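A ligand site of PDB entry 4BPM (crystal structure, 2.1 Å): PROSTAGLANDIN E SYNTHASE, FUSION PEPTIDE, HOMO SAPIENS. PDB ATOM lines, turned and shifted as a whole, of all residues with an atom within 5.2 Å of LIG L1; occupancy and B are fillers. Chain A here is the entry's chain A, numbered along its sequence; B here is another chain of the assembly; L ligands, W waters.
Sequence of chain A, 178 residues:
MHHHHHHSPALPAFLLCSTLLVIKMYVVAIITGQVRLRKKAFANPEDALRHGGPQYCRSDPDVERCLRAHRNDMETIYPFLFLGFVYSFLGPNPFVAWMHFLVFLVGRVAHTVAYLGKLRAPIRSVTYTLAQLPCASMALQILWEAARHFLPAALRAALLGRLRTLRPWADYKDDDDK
OG of Ser 125 lies within hydrogen-bond range of N3 of LG2 L2.
A nitrogen (N1) of LIG L1 lies within salt-bridge range of the side-chain carboxylate (OE1) of Glu 75 (3.2 Å).
OG of Ser 125 sits close to S1 of LIG L1, at 3.2 Å.
The side-chain amide nitrogen (ND2) of Asn 72 sits at hydrogen-bond distance from an oxygen (O3) of LIG L1 (3.2 Å).
The guanidinium group (NE) of Arg 124 is in hydrogen-bond range of an oxygen (O4) of LIG L1 (2.9 Å).
O1 of LIG L1 lies within salt-bridge range of NH2 of Arg 36 of chain B.
OH of Tyr 115 sits at hydrogen-bond distance from O6 of LIG L1, at 2.5 Å.
NE2 of His 111 lies within hydrogen-bond range of O4 of LIG L1.
NH2 of Arg 71 lies within salt-bridge range of O6 of LIG L1.
S1 of LIG L1 lies close to N1 of LG2 L2 (3.7 Å).
OH of Tyr 115 sits at hydrogen-bond distance from NE of Arg 68 (3.0 Å).
The side-chain amide nitrogen (ND2) of Asn 44 of chain B lies within hydrogen-bond range of the side-chain hydroxyl (OH) of Tyr 115 (3.1 Å).
NH1 of Arg 71 lies within salt-bridge range of OE2 of Glu 75 (2.7 Å).
OD1 of Asn 72 sits close to NE2 of His 111 (3.4 Å).
The side-chain amide oxygen of Asn 44 of chain B lies within hydrogen-bond range of the guanidinium group of Arg 68 (2.7 Å).
Residues that only touch LIG L1: Tyr 128, Leu 67 of chain B, Thr 32 of chain B, Ala 29 of chain B and Arg 68.
Hydrophobic or aromatic side chains that line LIG L1: His 111, Tyr 115, Tyr 128 and Leu 67 of chain B.
Within 4 Å of LIG L1: Arg 68, Arg 71, Asn 72, Glu 75, His 111, Tyr 115, Arg 124, Ser 125, Tyr 128, Ala 29 of chain B, Thr 32 of chain B, Arg 36 of chain B and Leu 67 of chain B.
Water W3 lies within hydrogen-bond range of a nitrogen (N1) of LIG L1 (2.8 Å), a ring nitrogen (ND1) of His 70 of chain B (2.8 Å) and the side-chain hydroxyl (OG1) of Thr 32 of chain B (3.0 Å).
Water W2 lies within hydrogen-bond range of OE1 of Glu 75 (2.5 Å) and O3 of LIG L1 (2.9 Å).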
ATOM      1  N   ARG A  68      15.501 -24.794 -26.371  1.00  0.00           N
ATOM      2  CA  ARG A  68      16.490 -24.032 -25.625  1.00  0.00           C
ATOM      3  C   ARG A  68      15.951 -22.673 -25.205  1.00  0.00           C
ATOM      4  O   ARG A  68      16.188 -22.214 -24.083  1.00  0.00           O
ATOM      5  CB  ARG A  68      17.785 -23.865 -26.434  1.00  0.00           C
ATOM      6  CG  ARG A  68      18.628 -25.122 -26.535  1.00  0.00           C
ATOM      7  CD  ARG A  68      20.064 -24.814 -26.930  1.00  0.00           C
ATOM      8  NE  ARG A  68      20.161 -24.198 -28.258  1.00  0.00           N
ATOM      9  CZ  ARG A  68      20.099 -24.883 -29.399  1.00  0.00           C
ATOM     10  NH1 ARG A  68      19.950 -26.200 -29.377  1.00  0.00           N
ATOM     11  NH2 ARG A  68      20.193 -24.250 -30.557  1.00  0.00           N
ATOM     12  N   ALA A  69      15.210 -22.034 -26.105  1.00  0.00           N
ATOM     13  CA  ALA A  69      14.598 -20.740 -25.815  1.00  0.00           C
ATOM     14  C   ALA A  69      13.564 -20.884 -24.701  1.00  0.00           C
ATOM     15  O   ALA A  69      13.490 -20.047 -23.805  1.00  0.00           O
ATOM     16  CB  ALA A  69      13.947 -20.170 -27.064  1.00  0.00           C
ATOM     17  N   ARG A  71      13.472 -23.297 -22.386  1.00  0.00           N
ATOM     18  CA  ARG A  71      14.177 -23.611 -21.144  1.00  0.00           C
ATOM     19  C   ARG A  71      14.774 -22.353 -20.512  1.00  0.00           C
ATOM     20  O   ARG A  71      14.685 -22.167 -19.296  1.00  0.00           O
ATOM     21  CB  ARG A  71      15.272 -24.649 -21.368  1.00  0.00           C
ATOM     22  CG  ARG A  71      16.137 -24.868 -20.121  1.00  0.00           C
ATOM     23  CD  ARG A  71      17.214 -25.919 -20.335  1.00  0.00           C
ATOM     24  NE  ARG A  71      18.025 -25.656 -21.516  1.00  0.00           N
ATOM     25  CZ  ARG A  71      18.938 -24.696 -21.613  1.00  0.00           C
ATOM     26  NH1 ARG A  71      19.148 -23.877 -20.592  1.00  0.00           N
ATOM     27  NH2 ARG A  71      19.628 -24.549 -22.731  1.00  0.00           N
ATOM     28  N   ASN A  72      15.363 -21.504 -21.340  1.00  0.00           N
ATOM     29  CA  ASN A  72      15.954 -20.269 -20.849  1.00  0.00           C
ATOM     30  C   ASN A  72      14.902 -19.342 -20.243  1.00  0.00           C
ATOM     31  O   ASN A  72      15.156 -18.672 -19.243  1.00  0.00           O
ATOM     32  CB  ASN A  72      16.723 -19.537 -21.958  1.00  0.00           C
ATOM     33  CG  ASN A  72      17.575 -18.396 -21.420  1.00  0.00           C
ATOM     34  OD1 ASN A  72      17.117 -17.264 -21.298  1.00  0.00           O
ATOM     35  ND2 ASN A  72      18.825 -18.698 -21.095  1.00  0.00           N
ATOM     36  N   GLU A  75      14.245 -20.666 -16.922  1.00  0.00           N
ATOM     37  CA  GLU A  75      15.354 -20.370 -16.016  1.00  0.00           C
ATOM     38  C   GLU A  75      15.353 -18.918 -15.531  1.00  0.00           C
ATOM     39  O   GLU A  75      16.021 -18.580 -14.555  1.00  0.00           O
ATOM     40  CB  GLU A  75      16.696 -20.700 -16.682  1.00  0.00           C
ATOM     41  CG  GLU A  75      16.895 -22.189 -16.957  1.00  0.00           C
ATOM     42  CD  GLU A  75      18.141 -22.478 -17.769  1.00  0.00           C
ATOM     43  OE1 GLU A  75      18.839 -21.518 -18.168  1.00  0.00           O
ATOM     44  OE2 GLU A  75      18.433 -23.664 -18.012  1.00  0.00           O
ATOM     45  N   HIS A 111      15.208 -11.234 -26.015  1.00  0.00           N
ATOM     46  CA  HIS A 111      15.982 -12.474 -25.923  1.00  0.00           C
ATOM     47  C   HIS A 111      15.409 -13.545 -26.837  1.00  0.00           C
ATOM     48  O   HIS A 111      16.150 -14.212 -27.566  1.00  0.00           O
ATOM     49  CB  HIS A 111      16.028 -12.996 -24.481  1.00  0.00           C
ATOM     50  CG  HIS A 111      16.882 -14.208 -24.316  1.00  0.00           C
ATOM     51  ND1 HIS A 111      16.420 -15.496 -24.499  1.00  0.00           N
ATOM     52  CD2 HIS A 111      18.197 -14.325 -23.989  1.00  0.00           C
ATOM     53  CE1 HIS A 111      17.403 -16.348 -24.290  1.00  0.00           C
ATOM     54  NE2 HIS A 111      18.486 -15.675 -23.982  1.00  0.00           N
ATOM     55  N   TYR A 115      16.944 -15.212 -30.224  1.00  0.00           N
ATOM     56  CA  TYR A 115      17.166 -16.651 -30.180  1.00  0.00           C
ATOM     57  C   TYR A 115      16.526 -17.373 -31.359  1.00  0.00           C
ATOM     58  O   TYR A 115      17.202 -18.071 -32.114  1.00  0.00           O
ATOM     59  CB  TYR A 115      16.674 -17.260 -28.856  1.00  0.00           C
ATOM     60  CG  TYR A 115      17.557 -18.387 -28.352  1.00  0.00           C
ATOM     61  CD1 TYR A 115      18.385 -19.088 -29.212  1.00  0.00           C
ATOM     62  CD2 TYR A 115      17.563 -18.733 -27.001  1.00  0.00           C
ATOM     63  CE1 TYR A 115      19.191 -20.109 -28.754  1.00  0.00           C
ATOM     64  CE2 TYR A 115      18.370 -19.753 -26.543  1.00  0.00           C
ATOM     65  CZ  TYR A 115      19.179 -20.443 -27.413  1.00  0.00           C
ATOM     66  OH  TYR A 115      19.985 -21.462 -26.972  1.00  0.00           O
ATOM     67  N   ARG A 124      22.016 -11.966 -28.333  1.00  0.00           N
ATOM     68  CA  ARG A 124      21.176 -12.706 -27.399  1.00  0.00           C
ATOM     69  C   ARG A 124      21.758 -12.684 -25.988  1.00  0.00           C
ATOM     70  O   ARG A 124      21.039 -12.473 -25.017  1.00  0.00           O
ATOM     71  CB  ARG A 124      21.011 -14.162 -27.862  1.00  0.00           C
ATOM     72  CG  ARG A 124      20.019 -14.962 -27.034  1.00  0.00           C
ATOM     73  CD  ARG A 124      20.186 -16.463 -27.247  1.00  0.00           C
ATOM     74  NE  ARG A 124      21.424 -16.977 -26.654  1.00  0.00           N
ATOM     75  CZ  ARG A 124      22.502 -17.311 -27.348  1.00  0.00           C
ATOM     76  NH1 ARG A 124      22.517 -17.181 -28.664  1.00  0.00           N
ATOM     77  NH2 ARG A 124      23.577 -17.780 -26.710  1.00  0.00           N
ATOM     78  N   SER A 125      23.061 -12.915 -25.899  1.00  0.00           N
ATOM     79  CA  SER A 125      23.754 -12.968 -24.612  1.00  0.00           C
ATOM     80  C   SER A 125      23.654 -11.632 -23.888  1.00  0.00           C
ATOM     81  O   SER A 125      23.557 -11.580 -22.657  1.00  0.00           O
ATOM     82  CB  SER A 125      25.221 -13.362 -24.808  1.00  0.00           C
ATOM     83  OG  SER A 125      25.812 -13.802 -23.596  1.00  0.00           O
ATOM     84  N   TYR A 128      20.132 -11.188 -22.451  1.00  0.00           N
ATOM     85  CA  TYR A 128      20.028 -12.023 -21.251  1.00  0.00           C
ATOM     86  C   TYR A 128      20.526 -11.258 -20.038  1.00  0.00           C
ATOM     87  O   TYR A 128      19.846 -11.175 -19.017  1.00  0.00           O
ATOM     88  CB  TYR A 128      20.816 -13.320 -21.408  1.00  0.00           C
ATOM     89  CG  TYR A 128      20.986 -14.073 -20.101  1.00  0.00           C
ATOM     90  CD1 TYR A 128      19.942 -14.835 -19.582  1.00  0.00           C
ATOM     91  CD2 TYR A 128      22.186 -14.026 -19.402  1.00  0.00           C
ATOM     92  CE1 TYR A 128      20.087 -15.514 -18.389  1.00  0.00           C
ATOM     93  CE2 TYR A 128      22.339 -14.705 -18.203  1.00  0.00           C
ATOM     94  CZ  TYR A 128      21.287 -15.444 -17.711  1.00  0.00           C
ATOM     95  OH  TYR A 128      21.438 -16.129 -16.524  1.00  0.00           O
ATOM     96  N   ALA B  29      23.872 -20.684 -13.405  1.00  0.00           N
ATOM     97  CA  ALA B  29      23.781 -20.151 -14.753  1.00  0.00           C
ATOM     98  C   ALA B  29      25.086 -19.509 -15.186  1.00  0.00           C
ATOM     99  O   ALA B  29      25.565 -19.727 -16.302  1.00  0.00           O
ATOM    100  CB  ALA B  29      22.639 -19.145 -14.852  1.00  0.00           C
ATOM    101  N   THR B  32      27.686 -22.113 -15.743  1.00  0.00           N
ATOM    102  CA  THR B  32      27.397 -22.767 -17.020  1.00  0.00           C
ATOM    103  C   THR B  32      27.995 -22.003 -18.188  1.00  0.00           C
ATOM    104  O   THR B  32      28.592 -22.592 -19.089  1.00  0.00           O
ATOM    105  CB  THR B  32      25.871 -22.940 -17.238  1.00  0.00           C
ATOM    106  OG1 THR B  32      25.313 -23.709 -16.158  1.00  0.00           O
ATOM    107  CG2 THR B  32      25.600 -23.667 -18.546  1.00  0.00           C
ATOM    108  N   GLY B  33      27.837 -20.688 -18.181  1.00  0.00           N
ATOM    109  CA  GLY B  33      28.388 -19.838 -19.230  1.00  0.00           C
ATOM    110  C   GLY B  33      29.903 -19.856 -19.276  1.00  0.00           C
ATOM    111  O   GLY B  33      30.495 -19.906 -20.351  1.00  0.00           O
ATOM    112  N   ARG B  36      31.186 -23.032 -20.686  1.00  0.00           N
ATOM    113  CA  ARG B  36      31.014 -22.953 -22.129  1.00  0.00           C
ATOM    114  C   ARG B  36      32.178 -22.218 -22.790  1.00  0.00           C
ATOM    115  O   ARG B  36      32.690 -22.649 -23.819  1.00  0.00           O
ATOM    116  CB  ARG B  36      29.698 -22.259 -22.505  1.00  0.00           C
ATOM    117  CG  ARG B  36      28.462 -23.119 -22.355  1.00  0.00           C
ATOM    118  CD  ARG B  36      27.268 -22.471 -23.044  1.00  0.00           C
ATOM    119  NE  ARG B  36      26.036 -23.221 -22.831  1.00  0.00           N
ATOM    120  CZ  ARG B  36      25.675 -24.289 -23.542  1.00  0.00           C
ATOM    121  NH1 ARG B  36      26.468 -24.740 -24.510  1.00  0.00           N
ATOM    122  NH2 ARG B  36      24.544 -24.910 -23.281  1.00  0.00           N
ATOM    123  N   ALA B  43      26.025 -23.990 -27.755  1.00  0.00           N
ATOM    124  CA  ALA B  43      24.821 -24.673 -28.186  1.00  0.00           C
ATOM    125  C   ALA B  43      24.351 -24.152 -29.540  1.00  0.00           C
ATOM    126  O   ALA B  43      23.656 -24.846 -30.274  1.00  0.00           O
ATOM    127  CB  ALA B  43      23.719 -24.512 -27.144  1.00  0.00           C
ATOM    128  N   ASN B  44      24.741 -22.925 -29.863  1.00  0.00           N
ATOM    129  CA  ASN B  44      24.328 -22.297 -31.107  1.00  0.00           C
ATOM    130  C   ASN B  44      25.506 -21.959 -32.020  1.00  0.00           C
ATOM    131  O   ASN B  44      26.546 -21.491 -31.554  1.00  0.00           O
ATOM    132  CB  ASN B  44      23.507 -21.041 -30.814  1.00  0.00           C
ATOM    133  CG  ASN B  44      22.394 -21.289 -29.816  1.00  0.00           C
ATOM    134  OD1 ASN B  44      21.381 -21.912 -30.142  1.00  0.00           O
ATOM    135  ND2 ASN B  44      22.570 -20.801 -28.598  1.00  0.00           N
ATOM    136  N   LEU B  67      24.015 -28.108 -16.885  1.00  0.00           N
ATOM    137  CA  LEU B  67      22.614 -28.035 -17.292  1.00  0.00           C
ATOM    138  C   LEU B  67      21.730 -28.994 -16.487  1.00  0.00           C
ATOM    139  O   LEU B  67      20.581 -28.668 -16.188  1.00  0.00           O
ATOM    140  CB  LEU B  67      22.460 -28.323 -18.792  1.00  0.00           C
ATOM    141  CG  LEU B  67      22.963 -27.238 -19.740  1.00  0.00           C
ATOM    142  CD1 LEU B  67      22.813 -27.667 -21.190  1.00  0.00           C
ATOM    143  CD2 LEU B  67      22.225 -25.933 -19.500  1.00  0.00           C
ATOM    144  N   HIS B  70      21.210 -27.431 -13.079  1.00  0.00           N
ATOM    145  CA  HIS B  70      20.267 -26.328 -13.191  1.00  0.00           C
ATOM    146  C   HIS B  70      18.835 -26.838 -13.335  1.00  0.00           C
ATOM    147  O   HIS B  70      17.916 -26.301 -12.719  1.00  0.00           O
ATOM    148  CB  HIS B  70      20.623 -25.420 -14.373  1.00  0.00           C
ATOM    149  CG  HIS B  70      20.064 -24.037 -14.270  1.00  0.00           C
ATOM    150  ND1 HIS B  70      20.385 -23.029 -15.162  1.00  0.00           N
ATOM    151  CD2 HIS B  70      19.213 -23.488 -13.374  1.00  0.00           C
ATOM    152  CE1 HIS B  70      19.753 -21.925 -14.816  1.00  0.00           C
ATOM    153  NE2 HIS B  70      19.035 -22.167 -13.732  1.00  0.00           N
HETATM  154  N1  LIG L   1      21.497 -22.615 -19.533  1.00  0.00           N
HETATM  155  C1  LIG L   1      22.282 -21.447 -19.962  1.00  0.00           C
HETATM  156  C2  LIG L   1      23.250 -22.030 -21.014  1.00  0.00           C
HETATM  157  O1  LIG L   1      23.414 -23.226 -21.182  1.00  0.00           O
HETATM  158  O2  LIG L   1      23.856 -21.106 -21.706  1.00  0.00           O
HETATM  159  C3  LIG L   1      23.071 -20.788 -18.808  1.00  0.00           C
HETATM  160  C4  LIG L   1      23.650 -19.426 -19.186  1.00  0.00           C
HETATM  161  C5  LIG L   1      22.654 -18.549 -19.909  1.00  0.00           C
HETATM  162  O3  LIG L   1      21.521 -18.387 -19.471  1.00  0.00           O
HETATM  163  N2  LIG L   1      23.094 -17.966 -21.021  1.00  0.00           N
HETATM  164  C6  LIG L   1      22.256 -17.062 -21.793  1.00  0.00           C
HETATM  165  C7  LIG L   1      21.563 -17.767 -22.953  1.00  0.00           C
HETATM  166  O4  LIG L   1      20.892 -17.133 -23.760  1.00  0.00           O
HETATM  167  C8  LIG L   1      23.137 -15.961 -22.444  1.00  0.00           C
HETATM  168  S1  LIG L   1      24.502 -16.756 -23.328  1.00  0.00           S
HETATM  169  N3  LIG L   1      21.716 -19.090 -23.036  1.00  0.00           N
HETATM  170  C9  LIG L   1      21.105 -19.870 -24.094  1.00  0.00           C
HETATM  171  C10 LIG L   1      20.400 -21.096 -23.596  1.00  0.00           C
HETATM  172  O5  LIG L   1      20.095 -21.284 -22.436  1.00  0.00           O
HETATM  173  O6  LIG L   1      20.147 -21.936 -24.556  1.00  0.00           O
HETATM  174  O1  LG2 L   2      29.019 -16.434 -19.605  1.00  0.00           O
HETATM  175  C1  LG2 L   2      27.913 -16.199 -20.065  1.00  0.00           C
HETATM  176  C2  LG2 L   2      26.917 -15.296 -19.345  1.00  0.00           C
HETATM  177  C3  LG2 L   2      27.649 -14.375 -18.372  1.00  0.00           C
HETATM  178  C4  LG2 L   2      26.151 -14.440 -20.361  1.00  0.00           C
HETATM  179  C5  LG2 L   2      25.916 -16.158 -18.564  1.00  0.00           C
HETATM  180  N1  LG2 L   2      27.497 -16.694 -21.226  1.00  0.00           N
HETATM  181  C6  LG2 L   2      28.338 -17.533 -22.067  1.00  0.00           C
HETATM  182  C7  LG2 L   2      28.371 -17.083 -23.505  1.00  0.00           C
HETATM  183  C8  LG2 L   2      27.692 -17.768 -24.500  1.00  0.00           C
HETATM  184  C9  LG2 L   2      27.662 -17.301 -25.803  1.00  0.00           C
HETATM  185  C10 LG2 L   2      28.325 -16.131 -26.132  1.00  0.00           C
HETATM  186 CL1  LG2 L   2      28.228 -15.561 -27.767  1.00  0.00          CL
HETATM  187  C11 LG2 L   2      29.045 -15.922 -23.865  1.00  0.00           C
HETATM  188 CL2  LG2 L   2      29.958 -15.085 -22.669  1.00  0.00          CL
HETATM  189  C12 LG2 L   2      29.039 -15.405 -25.191  1.00  0.00           C
HETATM  190  N2  LG2 L   2      29.721 -14.199 -25.552  1.00  0.00           N
HETATM  191  C13 LG2 L   2      29.408 -13.000 -24.994  1.00  0.00           C
HETATM  192  N3  LG2 L   2      28.526 -12.758 -24.060  1.00  0.00           N
HETATM  193  C14 LG2 L   2      28.617 -11.376 -23.843  1.00  0.00           C
HETATM  194  C15 LG2 L   2      29.570 -10.812 -24.685  1.00  0.00           C
HETATM  195  N4  LG2 L   2      30.092 -11.865 -25.432  1.00  0.00           N
HETATM  196  C16 LG2 L   2      31.148 -11.735 -26.436  1.00  0.00           C
HETATM  197  C17 LG2 L   2      29.856  -9.451 -24.680  1.00  0.00           C
HETATM  198  C18 LG2 L   2      29.140  -8.666 -23.799  1.00  0.00           C
HETATM  199  O2  LG2 L   2      29.319  -7.316 -23.731  1.00  0.00           O
HETATM  200  C19 LG2 L   2      30.605  -6.779 -24.089  1.00  0.00           C
HETATM  201  C20 LG2 L   2      30.285  -5.284 -24.294  1.00  0.00           C
HETATM  202  O3  LG2 L   2      29.992  -4.642 -23.035  1.00  0.00           O
HETATM  203  C21 LG2 L   2      29.053  -5.164 -25.179  1.00  0.00           C
HETATM  204  C22 LG2 L   2      31.467  -4.543 -24.915  1.00  0.00           C
HETATM  205  C23 LG2 L   2      28.177  -9.199 -22.913  1.00  0.00           C
HETATM  206  C24 LG2 L   2      27.910 -10.567 -22.960  1.00  0.00           C
HETATM  207  C25 LG2 L   2      27.422  -8.414 -21.893  1.00  0.00           C
HETATM  208  O4  LG2 L   2      26.415  -8.882 -21.366  1.00  0.00           O
HETATM  209  N5  LG2 L   2      27.884  -7.206 -21.579  1.00  0.00           N
HETATM  210  C26 LG2 L   2      27.316  -6.360 -20.535  1.00  0.00           C
HETATM  211  C27 LG2 L   2      26.008  -5.629 -21.047  1.00  0.00           C
HETATM  212  F1  LG2 L   2      25.401  -4.948 -20.078  1.00  0.00           F
HETATM  213  F2  LG2 L   2      25.110  -6.481 -21.530  1.00  0.00           F
HETATM  214  F3  LG2 L   2      26.263  -4.755 -22.016  1.00  0.00           F
HETATM  215  O   HOH W   1      24.954 -19.702 -23.736  1.00  0.00           O
HETATM  216  O   HOH W   2      19.759 -19.340 -17.397  1.00  0.00           O
HETATM  217  O   HOH W   3      22.411 -23.643 -17.061  1.00  0.00           O
